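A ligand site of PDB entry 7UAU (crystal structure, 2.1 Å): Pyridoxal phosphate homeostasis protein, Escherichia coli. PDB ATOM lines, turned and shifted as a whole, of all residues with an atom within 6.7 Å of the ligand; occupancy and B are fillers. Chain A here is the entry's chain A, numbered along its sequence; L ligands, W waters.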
ATOM      1  N   LEU A  32     -12.853  -9.453  16.054  1.00  0.00           N
ATOM      2  CA  LEU A  32     -12.543  -9.046  17.416  1.00  0.00           C
ATOM      3  C   LEU A  32     -12.362  -7.524  17.432  1.00  0.00           C
ATOM      4  O   LEU A  32     -11.387  -7.005  16.864  1.00  0.00           O
ATOM      5  CB  LEU A  32     -11.272  -9.732  17.935  1.00  0.00           C
ATOM      6  CG  LEU A  32     -10.927  -9.336  19.375  1.00  0.00           C
ATOM      7  CD1 LEU A  32     -12.006  -9.860  20.310  1.00  0.00           C
ATOM      8  CD2 LEU A  32      -9.518  -9.783  19.815  1.00  0.00           C
ATOM      9  N   VAL A  34     -11.080  -4.385  18.983  1.00  0.00           N
ATOM     10  CA  VAL A  34     -10.007  -4.107  19.951  1.00  0.00           C
ATOM     11  C   VAL A  34     -10.238  -2.719  20.521  1.00  0.00           C
ATOM     12  O   VAL A  34     -10.116  -1.708  19.810  1.00  0.00           O
ATOM     13  CB  VAL A  34      -8.614  -4.240  19.320  1.00  0.00           C
ATOM     14  CG1 VAL A  34      -7.548  -3.749  20.294  1.00  0.00           C
ATOM     15  CG2 VAL A  34      -8.364  -5.693  18.933  1.00  0.00           C
ATOM     16  N   LYS A  36      -8.800  -1.353  23.385  1.00  0.00           N
ATOM     17  CA  LYS A  36      -7.793  -0.788  24.261  1.00  0.00           C
ATOM     18  C   LYS A  36      -7.698   0.716  24.053  1.00  0.00           C
ATOM     19  O   LYS A  36      -7.893   1.222  22.929  1.00  0.00           O
ATOM     20  CB  LYS A  36      -6.427  -1.458  24.039  1.00  0.00           C
ATOM     21  CG  LYS A  36      -5.836  -1.339  22.641  1.00  0.00           C
ATOM     22  CD  LYS A  36      -4.281  -1.254  22.730  1.00  0.00           C
ATOM     23  CE  LYS A  36      -3.621  -1.202  21.354  1.00  0.00           C
ATOM     24  NZ  LYS A  36      -3.454  -2.576  20.773  1.00  0.00           N
ATOM     25  N   ASN A  57      -5.904  -4.998  26.156  1.00  0.00           N
ATOM     26  CA  ASN A  57      -4.473  -5.237  26.284  1.00  0.00           C
ATOM     27  C   ASN A  57      -3.930  -5.013  27.687  1.00  0.00           C
ATOM     28  O   ASN A  57      -2.869  -5.565  28.011  1.00  0.00           O
ATOM     29  CB  ASN A  57      -3.680  -4.336  25.331  1.00  0.00           C
ATOM     30  CG  ASN A  57      -3.897  -4.690  23.871  1.00  0.00           C
ATOM     31  OD1 ASN A  57      -4.944  -4.385  23.297  1.00  0.00           O
ATOM     32  ND2 ASN A  57      -2.894  -5.331  23.262  1.00  0.00           N
ATOM     33  N   TYR A  58      -4.602  -4.229  28.522  1.00  0.00           N
ATOM     34  CA  TYR A  58      -4.099  -3.859  29.834  1.00  0.00           C
ATOM     35  C   TYR A  58      -5.107  -4.293  30.883  1.00  0.00           C
ATOM     36  O   TYR A  58      -6.308  -4.032  30.743  1.00  0.00           O
ATOM     37  CB  TYR A  58      -3.846  -2.355  29.887  1.00  0.00           C
ATOM     38  CG  TYR A  58      -3.050  -1.888  28.684  1.00  0.00           C
ATOM     39  CD1 TYR A  58      -1.736  -2.296  28.504  1.00  0.00           C
ATOM     40  CD2 TYR A  58      -3.629  -1.074  27.727  1.00  0.00           C
ATOM     41  CE1 TYR A  58      -1.004  -1.885  27.391  1.00  0.00           C
ATOM     42  CE2 TYR A  58      -2.912  -0.656  26.619  1.00  0.00           C
ATOM     43  CZ  TYR A  58      -1.601  -1.059  26.463  1.00  0.00           C
ATOM     44  OH  TYR A  58      -0.892  -0.641  25.349  1.00  0.00           O
ATOM     45  N   ILE A  82      -5.549  -9.637  25.056  1.00  0.00           N
ATOM     46  CA  ILE A  82      -4.635  -9.829  23.944  1.00  0.00           C
ATOM     47  C   ILE A  82      -3.309  -9.099  24.147  1.00  0.00           C
ATOM     48  O   ILE A  82      -2.524  -8.962  23.204  1.00  0.00           O
ATOM     49  CB  ILE A  82      -5.290  -9.415  22.616  1.00  0.00           C
ATOM     50  CG1 ILE A  82      -5.602  -7.914  22.619  1.00  0.00           C
ATOM     51  CG2 ILE A  82      -6.570 -10.231  22.356  1.00  0.00           C
ATOM     52  CD1 ILE A  82      -6.156  -7.422  21.277  1.00  0.00           C
ATOM     53  N   GLY A  83      -3.031  -8.617  25.367  1.00  0.00           N
ATOM     54  CA  GLY A  83      -1.775  -7.977  25.671  1.00  0.00           C
ATOM     55  C   GLY A  83      -0.809  -8.949  26.335  1.00  0.00           C
ATOM     56  O   GLY A  83      -1.190 -10.075  26.682  1.00  0.00           O
ATOM     57  N   THR A 102      -2.392 -14.748  24.620  1.00  0.00           N
ATOM     58  CA  THR A 102      -0.955 -14.505  24.766  1.00  0.00           C
ATOM     59  C   THR A 102      -0.279 -15.518  25.701  1.00  0.00           C
ATOM     60  O   THR A 102       0.608 -15.164  26.471  1.00  0.00           O
ATOM     61  CB  THR A 102      -0.714 -13.069  25.249  1.00  0.00           C
ATOM     62  OG1 THR A 102      -1.491 -12.819  26.423  1.00  0.00           O
ATOM     63  CG2 THR A 102      -1.123 -12.063  24.159  1.00  0.00           C
ATOM     64  N   MET A 164      -2.270 -17.659  18.153  1.00  0.00           N
ATOM     65  CA  MET A 164      -2.288 -16.242  17.842  1.00  0.00           C
ATOM     66  C   MET A 164      -0.892 -15.856  17.392  1.00  0.00           C
ATOM     67  O   MET A 164       0.099 -16.423  17.850  1.00  0.00           O
ATOM     68  CB  MET A 164      -2.726 -15.391  19.062  1.00  0.00           C
ATOM     69  CG  MET A 164      -2.929 -13.909  18.766  1.00  0.00           C
ATOM     70  SD  MET A 164      -1.415 -12.919  18.925  1.00  0.00           S
ATOM     71  CE  MET A 164      -1.290 -12.655  20.676  1.00  0.00           C
ATOM     72  N   ILE A 166       1.275 -12.023  16.205  1.00  0.00           N
ATOM     73  CA  ILE A 166       1.418 -10.655  15.725  1.00  0.00           C
ATOM     74  C   ILE A 166       2.630 -10.642  14.811  1.00  0.00           C
ATOM     75  O   ILE A 166       3.761 -10.466  15.294  1.00  0.00           O
ATOM     76  CB  ILE A 166       1.605  -9.645  16.871  1.00  0.00           C
ATOM     77  CG1 ILE A 166       0.544  -9.834  17.945  1.00  0.00           C
ATOM     78  CG2 ILE A 166       1.598  -8.222  16.328  1.00  0.00           C
ATOM     79  CD1 ILE A 166       0.963  -9.294  19.278  1.00  0.00           C
ATOM     80  N   GLY A 203      -4.323 -11.373  11.974  1.00  0.00           N
ATOM     81  CA  GLY A 203      -4.744 -10.364  11.022  1.00  0.00           C
ATOM     82  C   GLY A 203      -5.235  -9.100  11.679  1.00  0.00           C
ATOM     83  O   GLY A 203      -6.072  -9.114  12.589  1.00  0.00           O
ATOM     84  N   MET A 204      -4.717  -7.970  11.200  1.00  0.00           N
ATOM     85  CA  MET A 204      -5.188  -6.653  11.608  1.00  0.00           C
ATOM     86  C   MET A 204      -5.558  -5.868  10.361  1.00  0.00           C
ATOM     87  O   MET A 204      -5.556  -6.430   9.261  1.00  0.00           O
ATOM     88  CB  MET A 204      -4.114  -5.939  12.447  1.00  0.00           C
ATOM     89  CG  MET A 204      -3.778  -6.726  13.732  1.00  0.00           C
ATOM     90  SD  MET A 204      -2.367  -6.139  14.712  1.00  0.00           S
ATOM     91  CE  MET A 204      -1.073  -7.068  13.933  1.00  0.00           C
ATOM     92  N   SER A 205      -5.859  -4.569  10.507  1.00  0.00           N
ATOM     93  CA  SER A 205      -6.405  -3.799   9.378  1.00  0.00           C
ATOM     94  C   SER A 205      -5.530  -3.909   8.134  1.00  0.00           C
ATOM     95  O   SER A 205      -6.032  -4.136   7.030  1.00  0.00           O
ATOM     96  CB  SER A 205      -6.568  -2.344   9.757  1.00  0.00           C
ATOM     97  OG  SER A 205      -7.645  -2.181  10.656  1.00  0.00           O
ATOM     98  N   ASP A 206      -4.212  -3.790   8.306  1.00  0.00           N
ATOM     99  CA  ASP A 206      -3.313  -3.641   7.171  1.00  0.00           C
ATOM    100  C   ASP A 206      -3.006  -4.949   6.453  1.00  0.00           C
ATOM    101  O   ASP A 206      -2.644  -4.921   5.264  1.00  0.00           O
ATOM    102  CB  ASP A 206      -2.003  -2.992   7.618  1.00  0.00           C
ATOM    103  CG  ASP A 206      -2.208  -1.564   8.107  1.00  0.00           C
ATOM    104  OD1 ASP A 206      -3.237  -0.936   7.728  1.00  0.00           O
ATOM    105  OD2 ASP A 206      -1.356  -1.070   8.872  1.00  0.00           O
ATOM    106  N   ARG A 220      -8.263  -8.882  14.315  1.00  0.00           N
ATOM    107  CA  ARG A 220      -8.304  -7.963  15.455  1.00  0.00           C
ATOM    108  C   ARG A 220      -8.235  -6.542  14.921  1.00  0.00           C
ATOM    109  O   ARG A 220      -7.206  -6.125  14.382  1.00  0.00           O
ATOM    110  CB  ARG A 220      -7.135  -8.246  16.408  1.00  0.00           C
ATOM    111  CG  ARG A 220      -7.052  -9.687  16.883  1.00  0.00           C
ATOM    112  CD  ARG A 220      -5.908  -9.845  17.916  1.00  0.00           C
ATOM    113  NE  ARG A 220      -4.634  -9.381  17.356  1.00  0.00           N
ATOM    114  CZ  ARG A 220      -3.833 -10.121  16.598  1.00  0.00           C
ATOM    115  NH1 ARG A 220      -4.153 -11.383  16.321  1.00  0.00           N
ATOM    116  NH2 ARG A 220      -2.703  -9.610  16.121  1.00  0.00           N
ATOM    117  N   ILE A 221      -9.319  -5.775  15.099  1.00  0.00           N
ATOM    118  CA  ILE A 221      -9.429  -4.449  14.516  1.00  0.00           C
ATOM    119  C   ILE A 221      -9.726  -3.433  15.615  1.00  0.00           C
ATOM    120  O   ILE A 221     -10.710  -3.563  16.344  1.00  0.00           O
ATOM    121  CB  ILE A 221     -10.522  -4.406  13.422  1.00  0.00           C
ATOM    122  CG1 ILE A 221     -10.322  -5.532  12.391  1.00  0.00           C
ATOM    123  CG2 ILE A 221     -10.585  -3.026  12.798  1.00  0.00           C
ATOM    124  CD1 ILE A 221      -8.980  -5.485  11.648  1.00  0.00           C
ATOM    125  N   GLY A 222      -8.895  -2.395  15.704  1.00  0.00           N
ATOM    126  CA  GLY A 222      -9.143  -1.358  16.681  1.00  0.00           C
ATOM    127  C   GLY A 222      -9.473  -0.012  16.056  1.00  0.00           C
ATOM    128  O   GLY A 222     -10.632   0.428  16.075  1.00  0.00           O
ATOM    129  N   THR A 223      -8.453   0.626  15.489  1.00  0.00           N
ATOM    130  CA  THR A 223      -8.573   2.003  14.998  1.00  0.00           C
ATOM    131  C   THR A 223      -9.659   2.142  13.947  1.00  0.00           C
ATOM    132  O   THR A 223     -10.474   3.061  14.004  1.00  0.00           O
ATOM    133  CB  THR A 223      -7.226   2.468  14.434  1.00  0.00           C
ATOM    134  OG1 THR A 223      -6.287   2.562  15.510  1.00  0.00           O
ATOM    135  CG2 THR A 223      -7.368   3.816  13.767  1.00  0.00           C
ATOM    136  N   ALA A 224      -9.690   1.222  12.968  1.00  0.00           N
ATOM    137  CA  ALA A 224     -10.699   1.276  11.927  1.00  0.00           C
ATOM    138  C   ALA A 224     -12.122   1.175  12.475  1.00  0.00           C
ATOM    139  O   ALA A 224     -13.079   1.481  11.750  1.00  0.00           O
ATOM    140  CB  ALA A 224     -10.452   0.163  10.915  1.00  0.00           C
ATOM    141  N   ILE A 225     -12.290   0.751  13.717  1.00  0.00           N
ATOM    142  CA  ILE A 225     -13.609   0.710  14.344  1.00  0.00           C
ATOM    143  C   ILE A 225     -13.848   1.947  15.203  1.00  0.00           C
ATOM    144  O   ILE A 225     -14.898   2.587  15.114  1.00  0.00           O
ATOM    145  CB  ILE A 225     -13.773  -0.576  15.169  1.00  0.00           C
ATOM    146  CG1 ILE A 225     -13.884  -1.810  14.270  1.00  0.00           C
ATOM    147  CG2 ILE A 225     -14.991  -0.482  16.110  1.00  0.00           C
ATOM    148  CD1 ILE A 225     -13.872  -3.106  15.055  1.00  0.00           C
ATOM    149  N   GLY A 227     -11.612   4.717  15.832  1.00  0.00           N
ATOM    150  CA  GLY A 227     -10.977   5.978  15.544  1.00  0.00           C
ATOM    151  C   GLY A 227      -9.607   6.112  16.193  1.00  0.00           C
ATOM    152  O   GLY A 227      -9.096   5.204  16.856  1.00  0.00           O
HETATM  153  N1  LIG L   1      -4.190  -6.672  17.882  1.00  0.00           N
HETATM  154  C1  LIG L   1      -3.389  -6.403  18.972  1.00  0.00           C
HETATM  155  C2  LIG L   1      -2.602  -7.499  19.627  1.00  0.00           C
HETATM  156  C3  LIG L   1      -3.290  -5.110  19.462  1.00  0.00           C
HETATM  157  O1  LIG L   1      -2.467  -4.865  20.534  1.00  0.00           O
HETATM  158  C4  LIG L   1      -4.011  -4.076  18.853  1.00  0.00           C
HETATM  159  C5  LIG L   1      -3.873  -2.699  19.412  1.00  0.00           C
HETATM  160  C6  LIG L   1      -4.819  -4.354  17.755  1.00  0.00           C
HETATM  161  C7  LIG L   1      -4.904  -5.659  17.283  1.00  0.00           C
HETATM  162  C8  LIG L   1      -5.637  -3.291  17.037  1.00  0.00           C
HETATM  163  O2  LIG L   1      -4.850  -2.188  16.615  1.00  0.00           O
HETATM  164  P1  LIG L   1      -5.264  -1.171  15.418  1.00  0.00           P
HETATM  165  O3  LIG L   1      -4.138  -1.131  14.413  1.00  0.00           O
HETATM  166  O4  LIG L   1      -6.540  -1.625  14.735  1.00  0.00           O
HETATM  167  O5  LIG L   1      -5.542   0.190  15.989  1.00  0.00           O
HETATM  168  O   HOH W   1      -6.070  -3.592  13.153  1.00  0.00           O
HETATM  169  O   HOH W   2       0.010  -5.533  20.927  1.00  0.00           O
HETATM  170  O   HOH W   3      -7.723  -0.577  12.563  1.00  0.00           O
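The side-chain amino group (NZ) of Lys 36 is covalently linked to a carbon (C5) of the ligand, at 1.4 Å.
N of Thr 223 lies within hydrogen-bond range of O5 of the ligand (3.0 Å).
O1 of the ligand lies within hydrogen-bond range of ND2 of Asn 57 (2.8 Å).
The guanidinium group of Arg 220 lies within hydrogen-bond range of a nitrogen (N1) of the ligand.
OG1 of Thr 223 sits at hydrogen-bond distance from O5 of the ligand (2.5 Å).
N of Gly 222 sits at hydrogen-bond distance from O4 of the ligand (2.7 Å).
The backbone NH (N) of Ile 221 lies within hydrogen-bond range of the backbone carbonyl oxygen (O) of Leu 32, at 3.0 Å.
The backbone carbonyl oxygen (O) of Ile 221 sits at hydrogen-bond distance from the backbone NH (N) of Val 34 (2.8 Å).
The side-chain amino group of Lys 36 sits close to the side-chain amide oxygen of Asn 57, at 3.4 Å.
The guanidinium group of Arg 220 lies close to the side-chain sulfur of Met 204, at 3.8 Å.
The backbone NH (N) of Arg 220 lies within hydrogen-bond range of the backbone carbonyl oxygen (O) of Gly 203, 2.8 Å away.
SD of Met 204 sits close to N1 of the ligand.
CG1 of Val 34 touches C6 of the ligand (3.8 Å).
Ile 82 touches the ligand (CD1 to C1, 3.7 Å).
C of Ile 221 touches O4 of the ligand, at 3.8 Å.
Hydrophobic or aromatic side chains that line the ligand: Val 34, Ile 82 and Met 204.
Within 4 Å of the ligand: Val 34, Lys 36, Asn 57, Ile 82, Met 204, Arg 220, Ile 221, Gly 222 and Thr 223.
Water W1 lies within hydrogen-bond range of an oxygen (O4) of the ligand, the backbone NH of Ser 205 and the backbone carbonyl oxygen of Arg 220.
Water W3 lies within hydrogen-bond range of OG of Ser 205, O4 of the ligand, N of Ala 224 and N of Thr 223.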
